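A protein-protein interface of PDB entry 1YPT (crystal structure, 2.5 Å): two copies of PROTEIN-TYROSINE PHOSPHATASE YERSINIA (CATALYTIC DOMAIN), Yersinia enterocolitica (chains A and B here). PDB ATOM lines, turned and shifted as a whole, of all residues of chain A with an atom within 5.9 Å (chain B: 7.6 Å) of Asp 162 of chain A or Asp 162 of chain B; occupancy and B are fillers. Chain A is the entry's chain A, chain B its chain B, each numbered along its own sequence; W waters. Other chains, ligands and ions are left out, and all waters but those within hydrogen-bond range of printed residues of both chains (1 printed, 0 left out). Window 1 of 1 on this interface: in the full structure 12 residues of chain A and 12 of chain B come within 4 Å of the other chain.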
ATOM      1  N   LEU A 160     -24.957   8.540  16.597  1.00  0.00           N
ATOM      2  CA  LEU A 160     -25.546   8.748  17.897  1.00  0.00           C
ATOM      3  C   LEU A 160     -24.611   9.436  18.880  1.00  0.00           C
ATOM      4  O   LEU A 160     -25.006   9.840  19.981  1.00  0.00           O
ATOM      5  CB  LEU A 160     -25.957   7.426  18.426  1.00  0.00           C
ATOM      6  CG  LEU A 160     -27.093   6.651  17.738  1.00  0.00           C
ATOM      7  CD1 LEU A 160     -27.179   5.322  18.444  1.00  0.00           C
ATOM      8  CD2 LEU A 160     -28.435   7.349  17.816  1.00  0.00           C
ATOM      9  N   GLY A 161     -23.347   9.613  18.512  1.00  0.00           N
ATOM     10  CA  GLY A 161     -22.369  10.215  19.388  1.00  0.00           C
ATOM     11  C   GLY A 161     -21.171   9.283  19.448  1.00  0.00           C
ATOM     12  O   GLY A 161     -21.326   8.074  19.262  1.00  0.00           O
ATOM     13  N   ASP A 162     -19.963   9.825  19.627  1.00  0.00           N
ATOM     14  CA  ASP A 162     -18.755   9.041  19.806  1.00  0.00           C
ATOM     15  C   ASP A 162     -18.481   8.004  18.752  1.00  0.00           C
ATOM     16  O   ASP A 162     -17.911   6.950  19.019  1.00  0.00           O
ATOM     17  CB  ASP A 162     -18.797   8.364  21.197  1.00  0.00           C
ATOM     18  CG  ASP A 162     -18.422   9.327  22.296  1.00  0.00           C
ATOM     19  OD1 ASP A 162     -17.769  10.326  22.026  1.00  0.00           O
ATOM     20  OD2 ASP A 162     -18.759   9.092  23.439  1.00  0.00           O
ATOM     21  N   GLY A 163     -18.907   8.256  17.530  1.00  0.00           N
ATOM     22  CA  GLY A 163     -18.738   7.261  16.475  1.00  0.00           C
ATOM     23  C   GLY A 163     -19.714   6.076  16.485  1.00  0.00           C
ATOM     24  O   GLY A 163     -19.643   5.235  15.582  1.00  0.00           O
ATOM     25  N   ILE A 164     -20.632   5.917  17.450  1.00  0.00           N
ATOM     26  CA  ILE A 164     -21.618   4.855  17.420  1.00  0.00           C
ATOM     27  C   ILE A 164     -22.626   5.309  16.381  1.00  0.00           C
ATOM     28  O   ILE A 164     -23.016   6.482  16.349  1.00  0.00           O
ATOM     29  CB  ILE A 164     -22.328   4.707  18.754  1.00  0.00           C
ATOM     30  CG1 ILE A 164     -21.376   4.676  19.919  1.00  0.00           C
ATOM     31  CG2 ILE A 164     -23.055   3.372  18.752  1.00  0.00           C
ATOM     32  CD1 ILE A 164     -20.480   3.451  20.031  1.00  0.00           C
ATOM     33  N   PRO A 192     -20.292  -1.092  21.081  1.00  0.00           N
ATOM     34  CA  PRO A 192     -19.042  -1.605  21.615  1.00  0.00           C
ATOM     35  C   PRO A 192     -19.144  -2.897  22.415  1.00  0.00           C
ATOM     36  O   PRO A 192     -19.699  -2.987  23.504  1.00  0.00           O
ATOM     37  CB  PRO A 192     -18.502  -0.426  22.405  1.00  0.00           C
ATOM     38  CG  PRO A 192     -19.697   0.411  22.754  1.00  0.00           C
ATOM     39  CD  PRO A 192     -20.451   0.309  21.454  1.00  0.00           C
ATOM     40  N   THR A 195     -16.657  -2.131  25.951  1.00  0.00           N
ATOM     41  CA  THR A 195     -17.039  -1.142  26.934  1.00  0.00           C
ATOM     42  C   THR A 195     -18.534  -0.940  27.046  1.00  0.00           C
ATOM     43  O   THR A 195     -19.351  -1.486  26.287  1.00  0.00           O
ATOM     44  CB  THR A 195     -16.359   0.191  26.597  1.00  0.00           C
ATOM     45  OG1 THR A 195     -16.054   0.250  25.202  1.00  0.00           O
ATOM     46  CG2 THR A 195     -15.088   0.347  27.402  1.00  0.00           C
ATOM     47  N   ALA A 196     -18.888  -0.147  28.042  1.00  0.00           N
ATOM     48  CA  ALA A 196     -20.265   0.250  28.207  1.00  0.00           C
ATOM     49  C   ALA A 196     -20.478   1.539  27.413  1.00  0.00           C
ATOM     50  O   ALA A 196     -19.569   2.356  27.185  1.00  0.00           O
ATOM     51  CB  ALA A 196     -20.580   0.530  29.668  1.00  0.00           C
ATOM     52  N   VAL A 197     -21.724   1.724  27.001  1.00  0.00           N
ATOM     53  CA  VAL A 197     -22.107   2.879  26.252  1.00  0.00           C
ATOM     54  C   VAL A 197     -22.465   3.908  27.276  1.00  0.00           C
ATOM     55  O   VAL A 197     -23.048   3.572  28.288  1.00  0.00           O
ATOM     56  CB  VAL A 197     -23.261   2.479  25.362  1.00  0.00           C
ATOM     57  CG1 VAL A 197     -24.044   3.633  24.803  1.00  0.00           C
ATOM     58  CG2 VAL A 197     -22.618   1.758  24.213  1.00  0.00           C
ATOM     59  N   SER A 198     -22.033   5.136  27.052  1.00  0.00           N
ATOM     60  CA  SER A 198     -22.272   6.281  27.919  1.00  0.00           C
ATOM     61  C   SER A 198     -23.742   6.627  28.039  1.00  0.00           C
ATOM     62  O   SER A 198     -24.547   6.265  27.164  1.00  0.00           O
ATOM     63  CB  SER A 198     -21.517   7.472  27.361  1.00  0.00           C
ATOM     64  OG  SER A 198     -21.939   7.917  26.067  1.00  0.00           O
ATOM     65  N   VAL A 201     -24.750   8.775  24.709  1.00  0.00           N
ATOM     66  CA  VAL A 201     -25.178   7.991  23.551  1.00  0.00           C
ATOM     67  C   VAL A 201     -26.477   7.251  23.871  1.00  0.00           C
ATOM     68  O   VAL A 201     -27.325   7.159  22.979  1.00  0.00           O
ATOM     69  CB  VAL A 201     -24.093   6.973  23.179  1.00  0.00           C
ATOM     70  CG1 VAL A 201     -24.503   5.970  22.118  1.00  0.00           C
ATOM     71  CG2 VAL A 201     -22.943   7.800  22.642  1.00  0.00           C
ATOM     72  N   GLY B 159      -9.416   1.156  27.481  1.00  0.00           N
ATOM     73  CA  GLY B 159     -10.721   1.514  26.927  1.00  0.00           C
ATOM     74  C   GLY B 159     -11.199   2.807  27.565  1.00  0.00           C
ATOM     75  O   GLY B 159     -11.113   2.918  28.779  1.00  0.00           O
ATOM     76  N   LEU B 160     -11.690   3.814  26.864  1.00  0.00           N
ATOM     77  CA  LEU B 160     -12.118   5.031  27.519  1.00  0.00           C
ATOM     78  C   LEU B 160     -13.621   5.180  27.620  1.00  0.00           C
ATOM     79  O   LEU B 160     -14.155   5.975  28.400  1.00  0.00           O
ATOM     80  CB  LEU B 160     -11.568   6.198  26.778  1.00  0.00           C
ATOM     81  CG  LEU B 160     -10.081   6.410  26.776  1.00  0.00           C
ATOM     82  CD1 LEU B 160      -9.801   7.471  25.718  1.00  0.00           C
ATOM     83  CD2 LEU B 160      -9.566   6.773  28.184  1.00  0.00           C
ATOM     84  N   GLY B 161     -14.366   4.452  26.816  1.00  0.00           N
ATOM     85  CA  GLY B 161     -15.817   4.528  26.851  1.00  0.00           C
ATOM     86  C   GLY B 161     -16.262   4.513  25.409  1.00  0.00           C
ATOM     87  O   GLY B 161     -15.448   4.816  24.529  1.00  0.00           O
ATOM     88  N   ASP B 162     -17.477   4.036  25.152  1.00  0.00           N
ATOM     89  CA  ASP B 162     -18.042   3.961  23.826  1.00  0.00           C
ATOM     90  C   ASP B 162     -17.190   3.385  22.732  1.00  0.00           C
ATOM     91  O   ASP B 162     -17.312   3.789  21.585  1.00  0.00           O
ATOM     92  CB  ASP B 162     -18.499   5.357  23.425  1.00  0.00           C
ATOM     93  CG  ASP B 162     -19.818   5.756  24.071  1.00  0.00           C
ATOM     94  OD1 ASP B 162     -20.581   4.886  24.461  1.00  0.00           O
ATOM     95  OD2 ASP B 162     -20.109   6.933  24.183  1.00  0.00           O
ATOM     96  N   GLY B 163     -16.314   2.430  23.035  1.00  0.00           N
ATOM     97  CA  GLY B 163     -15.458   1.857  22.002  1.00  0.00           C
ATOM     98  C   GLY B 163     -14.207   2.665  21.694  1.00  0.00           C
ATOM     99  O   GLY B 163     -13.368   2.165  20.946  1.00  0.00           O
ATOM    100  N   ILE B 164     -13.981   3.872  22.226  1.00  0.00           N
ATOM    101  CA  ILE B 164     -12.781   4.678  21.964  1.00  0.00           C
ATOM    102  C   ILE B 164     -11.674   4.071  22.824  1.00  0.00           C
ATOM    103  O   ILE B 164     -11.887   3.732  23.999  1.00  0.00           O
ATOM    104  CB  ILE B 164     -12.993   6.124  22.395  1.00  0.00           C
ATOM    105  CG1 ILE B 164     -14.406   6.588  22.067  1.00  0.00           C
ATOM    106  CG2 ILE B 164     -11.921   6.957  21.764  1.00  0.00           C
ATOM    107  CD1 ILE B 164     -14.688   7.418  20.821  1.00  0.00           C
ATOM    108  N   MET B 165     -10.468   3.930  22.288  1.00  0.00           N
ATOM    109  CA  MET B 165      -9.361   3.283  22.990  1.00  0.00           C
ATOM    110  C   MET B 165      -8.146   4.183  22.937  1.00  0.00           C
ATOM    111  O   MET B 165      -7.866   4.816  21.909  1.00  0.00           O
ATOM    112  CB  MET B 165      -8.936   1.984  22.332  1.00  0.00           C
ATOM    113  CG  MET B 165     -10.049   1.010  21.976  1.00  0.00           C
ATOM    114  SD  MET B 165     -10.710   0.295  23.489  1.00  0.00           S
ATOM    115  CE  MET B 165      -9.303  -0.733  23.851  1.00  0.00           C
ATOM    116  N   ASN B 190      -8.545   5.725  17.773  1.00  0.00           N
ATOM    117  CA  ASN B 190      -9.774   5.734  17.005  1.00  0.00           C
ATOM    118  C   ASN B 190     -10.698   6.860  17.411  1.00  0.00           C
ATOM    119  O   ASN B 190     -11.922   6.678  17.491  1.00  0.00           O
ATOM    120  CB  ASN B 190     -10.484   4.404  17.190  1.00  0.00           C
ATOM    121  CG  ASN B 190     -10.933   4.157  18.627  1.00  0.00           C
ATOM    122  OD1 ASN B 190     -10.440   4.768  19.589  1.00  0.00           O
ATOM    123  ND2 ASN B 190     -11.847   3.211  18.805  1.00  0.00           N
ATOM    124  N   TRP B 191     -10.090   8.022  17.706  1.00  0.00           N
ATOM    125  CA  TRP B 191     -10.827   9.266  17.935  1.00  0.00           C
ATOM    126  C   TRP B 191     -11.743   9.395  16.709  1.00  0.00           C
ATOM    127  O   TRP B 191     -11.218   9.308  15.593  1.00  0.00           O
ATOM    128  CB  TRP B 191      -9.858  10.482  18.003  1.00  0.00           C
ATOM    129  CG  TRP B 191     -10.527  11.757  18.440  1.00  0.00           C
ATOM    130  CD1 TRP B 191     -11.399  12.405  17.603  1.00  0.00           C
ATOM    131  CD2 TRP B 191     -10.428  12.350  19.675  1.00  0.00           C
ATOM    132  NE1 TRP B 191     -11.881  13.409  18.316  1.00  0.00           N
ATOM    133  CE2 TRP B 191     -11.336  13.420  19.543  1.00  0.00           C
ATOM    134  CE3 TRP B 191      -9.733  12.176  20.869  1.00  0.00           C
ATOM    135  CZ2 TRP B 191     -11.551  14.300  20.585  1.00  0.00           C
ATOM    136  CZ3 TRP B 191      -9.949  13.072  21.917  1.00  0.00           C
ATOM    137  CH2 TRP B 191     -10.849  14.118  21.779  1.00  0.00           C
ATOM    138  N   PRO B 192     -13.075   9.511  16.839  1.00  0.00           N
ATOM    139  CA  PRO B 192     -13.987   9.662  15.709  1.00  0.00           C
ATOM    140  C   PRO B 192     -13.723  10.864  14.806  1.00  0.00           C
ATOM    141  O   PRO B 192     -13.806  12.016  15.207  1.00  0.00           O
ATOM    142  CB  PRO B 192     -15.369   9.649  16.379  1.00  0.00           C
ATOM    143  CG  PRO B 192     -15.126   9.948  17.829  1.00  0.00           C
ATOM    144  CD  PRO B 192     -13.814   9.258  18.064  1.00  0.00           C
ATOM    145  N   THR B 195     -17.730  12.581  14.261  1.00  0.00           N
ATOM    146  CA  THR B 195     -18.423  13.165  15.390  1.00  0.00           C
ATOM    147  C   THR B 195     -17.511  13.778  16.429  1.00  0.00           C
ATOM    148  O   THR B 195     -16.279  13.699  16.376  1.00  0.00           O
ATOM    149  CB  THR B 195     -19.300  12.123  16.100  1.00  0.00           C
ATOM    150  OG1 THR B 195     -18.936  10.802  15.702  1.00  0.00           O
ATOM    151  CG2 THR B 195     -20.757  12.435  15.800  1.00  0.00           C
ATOM    152  N   ALA B 196     -18.171  14.446  17.371  1.00  0.00           N
ATOM    153  CA  ALA B 196     -17.497  15.001  18.532  1.00  0.00           C
ATOM    154  C   ALA B 196     -17.422  13.881  19.570  1.00  0.00           C
ATOM    155  O   ALA B 196     -18.225  12.917  19.537  1.00  0.00           O
ATOM    156  CB  ALA B 196     -18.308  16.171  19.107  1.00  0.00           C
ATOM    157  N   VAL B 197     -16.467  14.025  20.489  1.00  0.00           N
ATOM    158  CA  VAL B 197     -16.326  13.060  21.565  1.00  0.00           C
ATOM    159  C   VAL B 197     -17.103  13.619  22.740  1.00  0.00           C
ATOM    160  O   VAL B 197     -16.951  14.808  23.012  1.00  0.00           O
ATOM    161  CB  VAL B 197     -14.829  12.873  21.870  1.00  0.00           C
ATOM    162  CG1 VAL B 197     -14.509  12.109  23.122  1.00  0.00           C
ATOM    163  CG2 VAL B 197     -14.321  12.011  20.739  1.00  0.00           C
ATOM    164  N   SER B 198     -17.923  12.794  23.415  1.00  0.00           N
ATOM    165  CA  SER B 198     -18.821  13.184  24.488  1.00  0.00           C
ATOM    166  C   SER B 198     -18.048  13.714  25.688  1.00  0.00           C
ATOM    167  O   SER B 198     -16.832  13.474  25.817  1.00  0.00           O
ATOM    168  CB  SER B 198     -19.649  11.955  24.897  1.00  0.00           C
ATOM    169  OG  SER B 198     -18.916  10.843  25.437  1.00  0.00           O
ATOM    170  N   SER B 199     -18.731  14.345  26.648  1.00  0.00           N
ATOM    171  CA  SER B 199     -18.018  14.767  27.825  1.00  0.00           C
ATOM    172  C   SER B 199     -17.599  13.576  28.633  1.00  0.00           C
ATOM    173  O   SER B 199     -16.494  13.577  29.169  1.00  0.00           O
ATOM    174  CB  SER B 199     -18.864  15.650  28.683  1.00  0.00           C
ATOM    175  OG  SER B 199     -20.152  15.113  28.867  1.00  0.00           O
ATOM    176  N   GLU B 200     -18.393  12.505  28.660  1.00  0.00           N
ATOM    177  CA  GLU B 200     -18.044  11.320  29.429  1.00  0.00           C
ATOM    178  C   GLU B 200     -16.734  10.718  28.994  1.00  0.00           C
ATOM    179  O   GLU B 200     -15.896  10.436  29.852  1.00  0.00           O
ATOM    180  CB  GLU B 200     -19.130  10.265  29.297  1.00  0.00           C
ATOM    181  CG  GLU B 200     -20.303  10.631  30.187  1.00  0.00           C
ATOM    182  CD  GLU B 200     -21.570   9.803  30.037  1.00  0.00           C
ATOM    183  OE1 GLU B 200     -21.671   8.764  30.685  1.00  0.00           O
ATOM    184  OE2 GLU B 200     -22.448  10.198  29.274  1.00  0.00           O
ATOM    185  N   VAL B 201     -16.512  10.547  27.689  1.00  0.00           N
ATOM    186  CA  VAL B 201     -15.242   9.983  27.238  1.00  0.00           C
ATOM    187  C   VAL B 201     -14.167  11.024  27.475  1.00  0.00           C
ATOM    188  O   VAL B 201     -13.072  10.631  27.886  1.00  0.00           O
ATOM    189  CB  VAL B 201     -15.267   9.613  25.737  1.00  0.00           C
ATOM    190  CG1 VAL B 201     -13.882   9.182  25.234  1.00  0.00           C
ATOM    191  CG2 VAL B 201     -16.265   8.474  25.581  1.00  0.00           C
ATOM    192  N   THR B 202     -14.417  12.328  27.275  1.00  0.00           N
ATOM    193  CA  THR B 202     -13.384  13.313  27.503  1.00  0.00           C
ATOM    194  C   THR B 202     -12.919  13.263  28.952  1.00  0.00           C
ATOM    195  O   THR B 202     -11.717  13.262  29.211  1.00  0.00           O
ATOM    196  CB  THR B 202     -13.925  14.692  27.136  1.00  0.00           C
ATOM    197  OG1 THR B 202     -14.228  14.643  25.768  1.00  0.00           O
ATOM    198  CG2 THR B 202     -12.939  15.790  27.286  1.00  0.00           C
ATOM    199  N   GLN B 249     -10.170  20.919  23.976  1.00  0.00           N
ATOM    200  CA  GLN B 249     -11.172  20.134  24.684  1.00  0.00           C
ATOM    201  C   GLN B 249     -10.546  19.357  25.847  1.00  0.00           C
ATOM    202  O   GLN B 249     -11.000  19.454  26.997  1.00  0.00           O
ATOM    203  CB  GLN B 249     -11.824  19.183  23.682  1.00  0.00           C
ATOM    204  CG  GLN B 249     -13.174  18.738  24.146  1.00  0.00           C
ATOM    205  CD  GLN B 249     -13.816  17.766  23.193  1.00  0.00           C
ATOM    206  OE1 GLN B 249     -13.969  18.023  21.997  1.00  0.00           O
ATOM    207  NE2 GLN B 249     -14.223  16.622  23.690  1.00  0.00           N
ATOM    208  N   LYS B 293     -20.970  21.048  29.158  1.00  0.00           N
ATOM    209  CA  LYS B 293     -21.619  19.930  29.807  1.00  0.00           C
ATOM    210  C   LYS B 293     -20.822  19.618  31.030  1.00  0.00           C
ATOM    211  O   LYS B 293     -21.392  19.518  32.110  1.00  0.00           O
ATOM    212  CB  LYS B 293     -21.646  18.696  28.951  1.00  0.00           C
ATOM    213  CG  LYS B 293     -22.415  18.759  27.628  1.00  0.00           C
ATOM    214  CD  LYS B 293     -21.963  17.498  26.875  1.00  0.00           C
ATOM    215  CE  LYS B 293     -22.142  17.435  25.350  1.00  0.00           C
ATOM    216  NZ  LYS B 293     -21.333  16.323  24.834  1.00  0.00           N
HETATM  217  O   HOH W   1     -13.657  -0.837  24.094  1.00  0.00           O
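Water W1 lies within hydrogen-bond range of OG1 of Thr 195 of chain A and SD of Met 165 of chain B.
CD1 of Ile 164 of chain B touches O of Asp 162 of chain A, at 3.7 Å. Asp 162 of chain A touches Ala 196 of chain B (N to O, 3.5 Å). Asp 162 of chain A touches Val 197 of chain B (OD1 to CA, 3.1 Å). Asp 162 of chain A touches Val 201 of chain B (OD2 to CG2, 3.3 Å). Asp 162 of chain B touches Ile 164 of chain A (O to CD1, 3.5 Å). Pro 192 of chain A touches Asp 162 of chain B (CG to C, 3.9 Å). Pro 192 of chain A touches Gly 163 of chain B (CB to N, 3.7 Å). CA of Val 197 of chain A touches OD1 of Asp 162 of chain B (3.1 Å). Glu 200 of chain B touches Ser 198 of chain A. OD2 of Asp 162 of chain B touches CG2 of Val 201 of chain A, at 3.3 Å.
Of the printed residues of chain B, Asp 162 of chain A touches Asp 162, Ile 164, Pro 192, Ala 196, Val 197, Ser 198 and Val 201. Of the printed residues of chain B, Gly 163 of chain A touches Pro 192 and Thr 195. Of the printed residues of chain B, Val 197 of chain A touches Asp 162 (3.1 Å). Of the printed residues of chain B, Ser 198 of chain A touches Asp 162 and Glu 200. Asp 162 of chain B touches just these residues of chain A: Asp 162 (2.7 Å), Ile 164 (3.5 Å), Pro 192 (3.9 Å), Ala 196 (3.4 Å), Val 197 (3.1 Å), Ser 198 (2.8 Å) and Val 201 (3.3 Å). Met 165 of chain B touches none of the printed residues of chain A. Of the printed residues of chain A, Ser 198 of chain B touches Asp 162 (2.7 Å). Of the printed residues of chain A, Glu 200 of chain B touches Ser 198. Gln 249 of chain B touches none of the printed residues of chain A. The nearest printed residue of chain B that does not touch Asp 162 of chain A is Thr 195 of chain B (4.2 Å). The nearest residue of chain A that does not touch Asp 162 of chain B is Thr 195 of chain A (4.04 Å). The nearest printed residue of chain A that does not touch Thr 195 of chain B is Asp 162 of chain A (4.2 Å).
Asp 162 of chain A touches its own counterpart, Asp 162 of chain B. Asp 162 of chain A touches Pro 192 of chain B, and with the chains exchanged Pro 192 of chain A touches Asp 162 of chain B. Asp 162 of chain A touches Val 197 of chain B, and with the chains exchanged Val 197 of chain A touches Asp 162 of chain B. Gly 163 of chain A touches Thr 195 of chain B, and with the chains exchanged Thr 195 of chain A touches Gly 163 of chain B. 11 positions are printed for both chains.
Printed residues of chain A that touch a printed residue of chain B: Asp 162, Gly 163, Ile 164, Pro 192, Thr 195, Ala 196, Val 197, Ser 198 and Val 201. Hydrophobic or aromatic side chains of chain A within 4 Å of the printed part of chain B: Ile 164, Pro 192, Val 197 and Val 201. Printed residues of chain B that touch a printed residue of chain A: Asp 162, Gly 163, Ile 164, Pro 192, Thr 195, Ala 196, Val 197, Ser 198, Glu 200 and Val 201.
The backbone NH (N) of Gly 163 of chain B is in hydrogen-bond range of the side-chain hydroxyl (OG1) of Thr 195 of chain A, at 3.1 Å. The backbone carbonyl oxygen of Ala 196 of chain A lies within hydrogen-bond range of the backbone NH of Asp 162 of chain B (3.4 Å). The side-chain carboxylate of Asp 162 of chain A lies close to the side-chain carboxylate of Asp 162 of chain B (2.7 Å). The side-chain carboxylate (OD2) of Asp 162 of chain B is in hydrogen-bond range of the side-chain hydroxyl (OG) of Ser 198 of chain A (2.8 Å). The side-chain hydroxyl (OG1) of Thr 195 of chain B is in hydrogen-bond range of the backbone NH (N) of Gly 163 of chain A, 3.1 Å away. The side-chain carboxylate of Asp 162 of chain A sits at hydrogen-bond distance from the side-chain hydroxyl of Ser 198 of chain B, at 2.7 Å.
O of Gly 163 of chain B lies within hydrogen-bond range of ND2 of Asn 190 of chain B. N of Val 201 of chain B lies within hydrogen-bond range of OG of Ser 198 of chain B. O of Val 197 of chain B sits at hydrogen-bond distance from NE2 of Gln 249 of chain B (3.3 Å). OG1 of Thr 202 of chain B is in hydrogen-bond range of O of Ser 198 of chain B (2.9 Å). OG of Ser 198 of chain A lies within hydrogen-bond range of N of Val 201 of chain A, 3.2 Å away.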
